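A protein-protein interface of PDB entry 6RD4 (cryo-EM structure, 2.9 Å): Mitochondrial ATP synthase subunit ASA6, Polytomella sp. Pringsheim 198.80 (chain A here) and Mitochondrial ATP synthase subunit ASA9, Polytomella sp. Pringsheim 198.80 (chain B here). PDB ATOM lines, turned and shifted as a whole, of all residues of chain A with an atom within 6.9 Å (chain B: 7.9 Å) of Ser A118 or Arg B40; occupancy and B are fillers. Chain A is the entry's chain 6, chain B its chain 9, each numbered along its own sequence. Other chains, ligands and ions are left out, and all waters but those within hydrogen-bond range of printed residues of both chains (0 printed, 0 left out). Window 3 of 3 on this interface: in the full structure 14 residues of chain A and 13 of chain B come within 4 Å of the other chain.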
ATOM      1  N   ALA A 111      -3.866   0.100  19.250  1.00  0.00           N
ATOM      2  CA  ALA A 111      -4.314  -1.273  19.126  1.00  0.00           C
ATOM      3  C   ALA A 111      -5.623  -1.341  18.372  1.00  0.00           C
ATOM      4  O   ALA A 111      -5.935  -2.361  17.759  1.00  0.00           O
ATOM      5  CB  ALA A 111      -4.462  -1.904  20.499  1.00  0.00           C
ATOM      6  N   LEU A 113      -6.463   0.961  15.963  1.00  0.00           N
ATOM      7  CA  LEU A 113      -6.124   1.235  14.578  1.00  0.00           C
ATOM      8  C   LEU A 113      -5.676  -0.024  13.866  1.00  0.00           C
ATOM      9  O   LEU A 113      -5.826  -0.136  12.651  1.00  0.00           O
ATOM     10  CB  LEU A 113      -5.028   2.286  14.517  1.00  0.00           C
ATOM     11  CG  LEU A 113      -5.354   3.760  14.363  1.00  0.00           C
ATOM     12  CD1 LEU A 113      -6.121   4.245  15.512  1.00  0.00           C
ATOM     13  CD2 LEU A 113      -4.059   4.486  14.329  1.00  0.00           C
ATOM     14  N   ILE A 114      -5.100  -0.964  14.599  1.00  0.00           N
ATOM     15  CA  ILE A 114      -4.703  -2.241  14.033  1.00  0.00           C
ATOM     16  C   ILE A 114      -5.912  -3.148  13.877  1.00  0.00           C
ATOM     17  O   ILE A 114      -6.061  -3.837  12.866  1.00  0.00           O
ATOM     18  CB  ILE A 114      -3.603  -2.844  14.921  1.00  0.00           C
ATOM     19  CG1 ILE A 114      -2.273  -2.186  14.596  1.00  0.00           C
ATOM     20  CG2 ILE A 114      -3.525  -4.332  14.813  1.00  0.00           C
ATOM     21  CD1 ILE A 114      -1.294  -2.287  15.679  1.00  0.00           C
ATOM     22  N   SER A 115      -6.814  -3.133  14.850  1.00  0.00           N
ATOM     23  CA  SER A 115      -7.994  -3.973  14.771  1.00  0.00           C
ATOM     24  C   SER A 115      -9.031  -3.430  13.814  1.00  0.00           C
ATOM     25  O   SER A 115      -9.974  -4.144  13.481  1.00  0.00           O
ATOM     26  CB  SER A 115      -8.614  -4.134  16.143  1.00  0.00           C
ATOM     27  OG  SER A 115      -7.717  -4.806  16.993  1.00  0.00           O
ATOM     28  N   PHE A 116      -8.902  -2.182  13.386  1.00  0.00           N
ATOM     29  CA  PHE A 116      -9.804  -1.651  12.378  1.00  0.00           C
ATOM     30  C   PHE A 116      -9.334  -1.975  10.977  1.00  0.00           C
ATOM     31  O   PHE A 116     -10.153  -2.078  10.068  1.00  0.00           O
ATOM     32  CB  PHE A 116      -9.948  -0.150  12.547  1.00  0.00           C
ATOM     33  CG  PHE A 116     -10.931   0.239  13.591  1.00  0.00           C
ATOM     34  CD1 PHE A 116     -11.931  -0.622  13.967  1.00  0.00           C
ATOM     35  CD2 PHE A 116     -10.849   1.462  14.204  1.00  0.00           C
ATOM     36  CE1 PHE A 116     -12.834  -0.259  14.926  1.00  0.00           C
ATOM     37  CE2 PHE A 116     -11.741   1.815  15.165  1.00  0.00           C
ATOM     38  CZ  PHE A 116     -12.739   0.958  15.522  1.00  0.00           C
ATOM     39  N   SER A 117      -8.035  -2.168  10.779  1.00  0.00           N
ATOM     40  CA  SER A 117      -7.552  -2.638   9.493  1.00  0.00           C
ATOM     41  C   SER A 117      -7.879  -4.097   9.256  1.00  0.00           C
ATOM     42  O   SER A 117      -7.771  -4.566   8.125  1.00  0.00           O
ATOM     43  CB  SER A 117      -6.052  -2.455   9.399  1.00  0.00           C
ATOM     44  OG  SER A 117      -5.696  -1.149   9.776  1.00  0.00           O
ATOM     45  N   SER A 118      -8.255  -4.826  10.291  1.00  0.00           N
ATOM     46  CA  SER A 118      -8.492  -6.247  10.193  1.00  0.00           C
ATOM     47  C   SER A 118      -9.941  -6.626  10.389  1.00  0.00           C
ATOM     48  O   SER A 118     -10.257  -7.814  10.366  1.00  0.00           O
ATOM     49  CB  SER A 118      -7.637  -6.989  11.219  1.00  0.00           C
ATOM     50  OG  SER A 118      -6.317  -7.167  10.735  1.00  0.00           O
ATOM     51  N   LEU A 119     -10.828  -5.664  10.586  1.00  0.00           N
ATOM     52  CA  LEU A 119     -12.213  -6.002  10.852  1.00  0.00           C
ATOM     53  C   LEU A 119     -13.183  -5.234   9.978  1.00  0.00           C
ATOM     54  O   LEU A 119     -14.308  -5.689   9.762  1.00  0.00           O
ATOM     55  CB  LEU A 119     -12.544  -5.747  12.311  1.00  0.00           C
ATOM     56  CG  LEU A 119     -12.026  -6.812  13.253  1.00  0.00           C
ATOM     57  CD1 LEU A 119     -12.325  -6.410  14.669  1.00  0.00           C
ATOM     58  CD2 LEU A 119     -12.671  -8.129  12.918  1.00  0.00           C
ATOM     59  N   ILE A 120     -12.792  -4.064   9.504  1.00  0.00           N
ATOM     60  CA  ILE A 120     -13.711  -3.278   8.686  1.00  0.00           C
ATOM     61  C   ILE A 120     -13.783  -3.899   7.299  1.00  0.00           C
ATOM     62  O   ILE A 120     -12.734  -4.143   6.685  1.00  0.00           O
ATOM     63  CB  ILE A 120     -13.250  -1.832   8.612  1.00  0.00           C
ATOM     64  CG1 ILE A 120     -13.328  -1.184   9.979  1.00  0.00           C
ATOM     65  CG2 ILE A 120     -14.128  -1.059   7.685  1.00  0.00           C
ATOM     66  CD1 ILE A 120     -12.790   0.208  10.004  1.00  0.00           C
ATOM     67  N   PRO A 121     -14.958  -4.220   6.790  1.00  0.00           N
ATOM     68  CA  PRO A 121     -15.034  -4.696   5.410  1.00  0.00           C
ATOM     69  C   PRO A 121     -14.868  -3.541   4.450  1.00  0.00           C
ATOM     70  O   PRO A 121     -15.811  -2.798   4.192  1.00  0.00           O
ATOM     71  CB  PRO A 121     -16.426  -5.317   5.335  1.00  0.00           C
ATOM     72  CG  PRO A 121     -17.201  -4.662   6.405  1.00  0.00           C
ATOM     73  CD  PRO A 121     -16.265  -4.227   7.461  1.00  0.00           C
ATOM     74  N   PHE A 122     -13.681  -3.389   3.882  1.00  0.00           N
ATOM     75  CA  PHE A 122     -13.378  -2.164   3.171  1.00  0.00           C
ATOM     76  C   PHE A 122     -13.994  -2.109   1.792  1.00  0.00           C
ATOM     77  O   PHE A 122     -14.102  -1.025   1.227  1.00  0.00           O
ATOM     78  CB  PHE A 122     -11.880  -1.985   3.063  1.00  0.00           C
ATOM     79  CG  PHE A 122     -11.250  -1.545   4.318  1.00  0.00           C
ATOM     80  CD1 PHE A 122     -11.448  -0.273   4.786  1.00  0.00           C
ATOM     81  CD2 PHE A 122     -10.448  -2.397   5.032  1.00  0.00           C
ATOM     82  CE1 PHE A 122     -10.859   0.140   5.940  1.00  0.00           C
ATOM     83  CE2 PHE A 122      -9.854  -1.985   6.181  1.00  0.00           C
ATOM     84  CZ  PHE A 122     -10.061  -0.716   6.635  1.00  0.00           C
ATOM     85  N   TYR B  14       3.085  -7.740   3.529  1.00  0.00           N
ATOM     86  CA  TYR B  14       2.967  -8.065   4.941  1.00  0.00           C
ATOM     87  C   TYR B  14       1.538  -7.857   5.434  1.00  0.00           C
ATOM     88  O   TYR B  14       1.058  -8.606   6.292  1.00  0.00           O
ATOM     89  CB  TYR B  14       3.950  -7.236   5.770  1.00  0.00           C
ATOM     90  CG  TYR B  14       3.603  -7.211   7.234  1.00  0.00           C
ATOM     91  CD1 TYR B  14       3.701  -8.353   8.013  1.00  0.00           C
ATOM     92  CD2 TYR B  14       3.139  -6.054   7.829  1.00  0.00           C
ATOM     93  CE1 TYR B  14       3.353  -8.338   9.338  1.00  0.00           C
ATOM     94  CE2 TYR B  14       2.791  -6.031   9.151  1.00  0.00           C
ATOM     95  CZ  TYR B  14       2.901  -7.171   9.897  1.00  0.00           C
ATOM     96  OH  TYR B  14       2.556  -7.130  11.219  1.00  0.00           O
ATOM     97  N   PHE B  15       0.838  -6.868   4.882  1.00  0.00           N
ATOM     98  CA  PHE B  15      -0.528  -6.597   5.306  1.00  0.00           C
ATOM     99  C   PHE B  15      -1.477  -7.687   4.844  1.00  0.00           C
ATOM    100  O   PHE B  15      -2.322  -8.147   5.613  1.00  0.00           O
ATOM    101  CB  PHE B  15      -0.980  -5.242   4.767  1.00  0.00           C
ATOM    102  CG  PHE B  15      -2.273  -4.765   5.323  1.00  0.00           C
ATOM    103  CD1 PHE B  15      -3.447  -4.941   4.627  1.00  0.00           C
ATOM    104  CD2 PHE B  15      -2.318  -4.118   6.528  1.00  0.00           C
ATOM    105  CE1 PHE B  15      -4.634  -4.514   5.135  1.00  0.00           C
ATOM    106  CE2 PHE B  15      -3.507  -3.685   7.032  1.00  0.00           C
ATOM    107  CZ  PHE B  15      -4.665  -3.883   6.334  1.00  0.00           C
ATOM    108  N   ALA B  20      -0.264 -14.854  10.090  1.00  0.00           N
ATOM    109  CA  ALA B  20       0.112 -15.818  11.106  1.00  0.00           C
ATOM    110  C   ALA B  20      -1.075 -16.574  11.670  1.00  0.00           C
ATOM    111  O   ALA B  20      -0.880 -17.434  12.525  1.00  0.00           O
ATOM    112  CB  ALA B  20       0.862 -15.133  12.243  1.00  0.00           C
ATOM    113  N   TYR B  21      -2.297 -16.273  11.245  1.00  0.00           N
ATOM    114  CA  TYR B  21      -3.419 -17.095  11.662  1.00  0.00           C
ATOM    115  C   TYR B  21      -3.452 -18.415  10.923  1.00  0.00           C
ATOM    116  O   TYR B  21      -4.010 -19.385  11.437  1.00  0.00           O
ATOM    117  CB  TYR B  21      -4.728 -16.357  11.447  1.00  0.00           C
ATOM    118  CG  TYR B  21      -5.942 -17.140  11.861  1.00  0.00           C
ATOM    119  CD1 TYR B  21      -6.161 -17.457  13.180  1.00  0.00           C
ATOM    120  CD2 TYR B  21      -6.853 -17.579  10.924  1.00  0.00           C
ATOM    121  CE1 TYR B  21      -7.267 -18.164  13.562  1.00  0.00           C
ATOM    122  CE2 TYR B  21      -7.961 -18.288  11.292  1.00  0.00           C
ATOM    123  CZ  TYR B  21      -8.161 -18.580  12.612  1.00  0.00           C
ATOM    124  OH  TYR B  21      -9.270 -19.293  12.991  1.00  0.00           O
ATOM    125  N   LEU B  30      -8.069 -21.917  17.777  1.00  0.00           N
ATOM    126  CA  LEU B  30      -8.975 -20.781  17.735  1.00  0.00           C
ATOM    127  C   LEU B  30     -10.185 -21.094  16.871  1.00  0.00           C
ATOM    128  O   LEU B  30     -10.067 -21.743  15.829  1.00  0.00           O
ATOM    129  CB  LEU B  30      -8.257 -19.534  17.221  1.00  0.00           C
ATOM    130  CG  LEU B  30      -7.379 -18.947  18.324  1.00  0.00           C
ATOM    131  CD1 LEU B  30      -6.302 -18.050  17.778  1.00  0.00           C
ATOM    132  CD2 LEU B  30      -8.245 -18.196  19.303  1.00  0.00           C
ATOM    133  N   LYS B  33     -11.747 -16.453  12.921  1.00  0.00           N
ATOM    134  CA  LYS B  33     -10.713 -15.431  12.844  1.00  0.00           C
ATOM    135  C   LYS B  33     -11.138 -14.140  13.514  1.00  0.00           C
ATOM    136  O   LYS B  33     -10.282 -13.322  13.855  1.00  0.00           O
ATOM    137  CB  LYS B  33     -10.322 -15.138  11.394  1.00  0.00           C
ATOM    138  CG  LYS B  33      -8.900 -14.650  11.275  1.00  0.00           C
ATOM    139  CD  LYS B  33      -8.525 -14.231   9.886  1.00  0.00           C
ATOM    140  CE  LYS B  33      -7.095 -13.722   9.886  1.00  0.00           C
ATOM    141  NZ  LYS B  33      -6.645 -13.272   8.543  1.00  0.00           N
ATOM    142  N   GLY B  34     -12.432 -13.956  13.736  1.00  0.00           N
ATOM    143  CA  GLY B  34     -12.905 -12.806  14.471  1.00  0.00           C
ATOM    144  C   GLY B  34     -12.544 -12.816  15.932  1.00  0.00           C
ATOM    145  O   GLY B  34     -12.646 -11.769  16.579  1.00  0.00           O
ATOM    146  N   GLN B  35     -12.147 -13.963  16.471  1.00  0.00           N
ATOM    147  CA  GLN B  35     -11.623 -14.036  17.819  1.00  0.00           C
ATOM    148  C   GLN B  35     -10.123 -14.266  17.861  1.00  0.00           C
ATOM    149  O   GLN B  35      -9.547 -14.249  18.946  1.00  0.00           O
ATOM    150  CB  GLN B  35     -12.346 -15.119  18.613  1.00  0.00           C
ATOM    151  CG  GLN B  35     -11.872 -16.518  18.362  1.00  0.00           C
ATOM    152  CD  GLN B  35     -12.463 -17.489  19.356  1.00  0.00           C
ATOM    153  OE1 GLN B  35     -13.537 -17.249  19.906  1.00  0.00           O
ATOM    154  NE2 GLN B  35     -11.761 -18.586  19.602  1.00  0.00           N
ATOM    155  N   TYR B  36      -9.503 -14.338  16.683  1.00  0.00           N
ATOM    156  CA  TYR B  36      -8.021 -14.354  16.639  1.00  0.00           C
ATOM    157  C   TYR B  36      -7.602 -12.883  16.702  1.00  0.00           C
ATOM    158  O   TYR B  36      -6.587 -12.564  17.345  1.00  0.00           O
ATOM    159  CB  TYR B  36      -7.487 -14.969  15.347  1.00  0.00           C
ATOM    160  CG  TYR B  36      -6.115 -14.466  14.982  1.00  0.00           C
ATOM    161  CD1 TYR B  36      -5.015 -14.764  15.769  1.00  0.00           C
ATOM    162  CD2 TYR B  36      -5.917 -13.665  13.872  1.00  0.00           C
ATOM    163  CE1 TYR B  36      -3.750 -14.297  15.452  1.00  0.00           C
ATOM    164  CE2 TYR B  36      -4.660 -13.190  13.542  1.00  0.00           C
ATOM    165  CZ  TYR B  36      -3.572 -13.507  14.333  1.00  0.00           C
ATOM    166  OH  TYR B  36      -2.333 -13.037  14.010  1.00  0.00           O
ATOM    167  N   VAL B  37      -8.389 -12.016  16.048  1.00  0.00           N
ATOM    168  CA  VAL B  37      -8.144 -10.580  16.057  1.00  0.00           C
ATOM    169  C   VAL B  37      -8.496  -9.999  17.413  1.00  0.00           C
ATOM    170  O   VAL B  37      -7.814  -9.107  17.918  1.00  0.00           O
ATOM    171  CB  VAL B  37      -8.941  -9.909  14.920  1.00  0.00           C
ATOM    172  CG1 VAL B  37      -8.711  -8.429  14.893  1.00  0.00           C
ATOM    173  CG2 VAL B  37      -8.546 -10.496  13.596  1.00  0.00           C
ATOM    174  N   ALA B  38      -9.512 -10.553  18.062  1.00  0.00           N
ATOM    175  CA  ALA B  38      -9.930 -10.056  19.359  1.00  0.00           C
ATOM    176  C   ALA B  38      -9.001 -10.458  20.489  1.00  0.00           C
ATOM    177  O   ALA B  38      -9.231 -10.026  21.616  1.00  0.00           O
ATOM    178  CB  ALA B  38     -11.338 -10.537  19.678  1.00  0.00           C
ATOM    179  N   LEU B  39      -7.995 -11.295  20.253  1.00  0.00           N
ATOM    180  CA  LEU B  39      -6.961 -11.500  21.250  1.00  0.00           C
ATOM    181  C   LEU B  39      -5.563 -11.239  20.731  1.00  0.00           C
ATOM    182  O   LEU B  39      -4.628 -11.205  21.532  1.00  0.00           O
ATOM    183  CB  LEU B  39      -7.038 -12.910  21.855  1.00  0.00           C
ATOM    184  CG  LEU B  39      -6.921 -14.191  21.048  1.00  0.00           C
ATOM    185  CD1 LEU B  39      -5.502 -14.723  21.041  1.00  0.00           C
ATOM    186  CD2 LEU B  39      -7.863 -15.211  21.632  1.00  0.00           C
ATOM    187  N   ARG B  40      -5.383 -11.060  19.430  1.00  0.00           N
ATOM    188  CA  ARG B  40      -4.193 -10.363  18.969  1.00  0.00           C
ATOM    189  C   ARG B  40      -4.244  -8.906  19.387  1.00  0.00           C
ATOM    190  O   ARG B  40      -3.205  -8.290  19.638  1.00  0.00           O
ATOM    191  CB  ARG B  40      -4.070 -10.487  17.460  1.00  0.00           C
ATOM    192  CG  ARG B  40      -2.923  -9.744  16.843  1.00  0.00           C
ATOM    193  CD  ARG B  40      -2.885 -10.013  15.388  1.00  0.00           C
ATOM    194  NE  ARG B  40      -2.326  -8.917  14.619  1.00  0.00           N
ATOM    195  CZ  ARG B  40      -3.048  -8.122  13.844  1.00  0.00           C
ATOM    196  NH1 ARG B  40      -2.457  -7.153  13.150  1.00  0.00           N
ATOM    197  NH2 ARG B  40      -4.357  -8.308  13.760  1.00  0.00           N
ATOM    198  N   HIS B  41      -5.451  -8.352  19.490  1.00  0.00           N
ATOM    199  CA  HIS B  41      -5.638  -7.015  20.033  1.00  0.00           C
ATOM    200  C   HIS B  41      -5.211  -6.947  21.487  1.00  0.00           C
ATOM    201  O   HIS B  41      -4.388  -6.110  21.861  1.00  0.00           O
ATOM    202  CB  HIS B  41      -7.099  -6.617  19.886  1.00  0.00           C
ATOM    203  CG  HIS B  41      -7.406  -5.247  20.381  1.00  0.00           C
ATOM    204  ND1 HIS B  41      -7.455  -4.152  19.553  1.00  0.00           N
ATOM    205  CD2 HIS B  41      -7.699  -4.796  21.618  1.00  0.00           C
ATOM    206  CE1 HIS B  41      -7.748  -3.083  20.264  1.00  0.00           C
ATOM    207  NE2 HIS B  41      -7.898  -3.447  21.520  1.00  0.00           N
ATOM    208  N   VAL B  42      -5.757  -7.829  22.321  1.00  0.00           N
ATOM    209  CA  VAL B  42      -5.400  -7.843  23.733  1.00  0.00           C
ATOM    210  C   VAL B  42      -3.977  -8.341  23.912  1.00  0.00           C
ATOM    211  O   VAL B  42      -3.298  -7.969  24.869  1.00  0.00           O
ATOM    212  CB  VAL B  42      -6.412  -8.699  24.504  1.00  0.00           C
ATOM    213  CG1 VAL B  42      -6.269  -8.496  25.976  1.00  0.00           C
ATOM    214  CG2 VAL B  42      -7.803  -8.345  24.076  1.00  0.00           C
ATOM    215  N   GLY B  43      -3.489  -9.158  22.985  1.00  0.00           N
ATOM    216  CA  GLY B  43      -2.093  -9.538  23.020  1.00  0.00           C
ATOM    217  C   GLY B  43      -1.165  -8.389  22.690  1.00  0.00           C
ATOM    218  O   GLY B  43      -0.062  -8.312  23.217  1.00  0.00           O
ATOM    219  N   PHE B  44      -1.593  -7.489  21.810  1.00  0.00           N
ATOM    220  CA  PHE B  44      -0.789  -6.311  21.496  1.00  0.00           C
ATOM    221  C   PHE B  44      -0.708  -5.370  22.684  1.00  0.00           C
ATOM    222  O   PHE B  44       0.307  -4.697  22.870  1.00  0.00           O
ATOM    223  CB  PHE B  44      -1.389  -5.592  20.287  1.00  0.00           C
ATOM    224  CG  PHE B  44      -0.651  -4.356  19.864  1.00  0.00           C
ATOM    225  CD1 PHE B  44       0.438  -4.435  19.037  1.00  0.00           C
ATOM    226  CD2 PHE B  44      -1.077  -3.109  20.263  1.00  0.00           C
ATOM    227  CE1 PHE B  44       1.096  -3.299  18.639  1.00  0.00           C
ATOM    228  CE2 PHE B  44      -0.415  -1.984  19.877  1.00  0.00           C
ATOM    229  CZ  PHE B  44       0.667  -2.078  19.064  1.00  0.00           C
ATOM    230  N   VAL B  45      -1.768  -5.304  23.484  1.00  0.00           N
ATOM    231  CA  VAL B  45      -1.773  -4.422  24.641  1.00  0.00           C
ATOM    232  C   VAL B  45      -0.891  -4.990  25.743  1.00  0.00           C
ATOM    233  O   VAL B  45      -0.090  -4.265  26.340  1.00  0.00           O
ATOM    234  CB  VAL B  45      -3.218  -4.192  25.112  1.00  0.00           C
ATOM    235  CG1 VAL B  45      -3.246  -3.376  26.358  1.00  0.00           C
ATOM    236  CG2 VAL B  45      -3.995  -3.498  24.047  1.00  0.00           C
ATOM    237  N   MET B  46      -0.995  -6.296  26.007  1.00  0.00           N
ATOM    238  CA  MET B  46      -0.205  -6.912  27.070  1.00  0.00           C
ATOM    239  C   MET B  46       1.272  -6.925  26.728  1.00  0.00           C
ATOM    240  O   MET B  46       2.115  -6.789  27.614  1.00  0.00           O
ATOM    241  CB  MET B  46      -0.674  -8.334  27.324  1.00  0.00           C
ATOM    242  CG  MET B  46      -2.044  -8.459  27.902  1.00  0.00           C
ATOM    243  SD  MET B  46      -2.329 -10.122  28.514  1.00  0.00           S
ATOM    244  CE  MET B  46      -1.730 -11.102  27.145  1.00  0.00           C
ATOM    245  N   VAL B  47       1.606  -7.102  25.455  1.00  0.00           N
ATOM    246  CA  VAL B  47       2.998  -6.995  25.044  1.00  0.00           C
ATOM    247  C   VAL B  47       3.467  -5.555  25.136  1.00  0.00           C
ATOM    248  O   VAL B  47       4.568  -5.281  25.619  1.00  0.00           O
ATOM    249  CB  VAL B  47       3.178  -7.576  23.633  1.00  0.00           C
ATOM    250  CG1 VAL B  47       4.529  -7.241  23.074  1.00  0.00           C
ATOM    251  CG2 VAL B  47       3.048  -9.071  23.688  1.00  0.00           C
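Printed residues of chain B within 4 Å of Ala A111: His B41 (3.0 Å), Phe B44 (3.6 Å) and Val B45 (3.9 Å).
Printed residues of chain B within 4 Å of Ile A114: Arg B40 (3.4 Å) and Phe B44 (3.9 Å).
Printed residues of chain B within 4 Å of Ser A115: His B41 (2.7 Å).
Of the printed residues of chain B, Ser A117 touches Phe B15 (3.6 Å).
Of chain B, only Arg B40 (3.8 Å) comes within 4 Å of Ser A118.
Lys B33 touches none of the printed residues of chain A.
Of chain A, only Ile A114 and Ser A118 come within 4 Å of Arg B40.
The backbone carbonyl oxygen of Ala A111 is in hydrogen-bond range of a ring nitrogen (ND1) of His B41, 3.0 Å away.
ND1 of His B41 is in hydrogen-bond range of OG of Ser A115, at 2.7 Å.
OG of Ser A115 is in hydrogen-bond range of O of Ala A111 (3.1 Å).
The side-chain hydroxyl (OG) of Ser A117 lies within hydrogen-bond range of the backbone carbonyl oxygen (O) of Leu A113, at 3.1 Å.
Among the printed residues, merely in contact across the chains: Ala A111 with Phe B44 (3.6 Å), Ala A111 with Val B45 (3.9 Å), Ile A114 with Arg B40 (3.4 Å), Ile A114 with Phe B44 (3.9 Å), Ser A117 with Phe B15 (3.6 Å) and Ser A118 with Arg B40 (3.8 Å).
Among the printed residues, no Asp or Glu carboxylate lies within 4 Å of a Lys or Arg side-chain nitrogen of the other chain.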
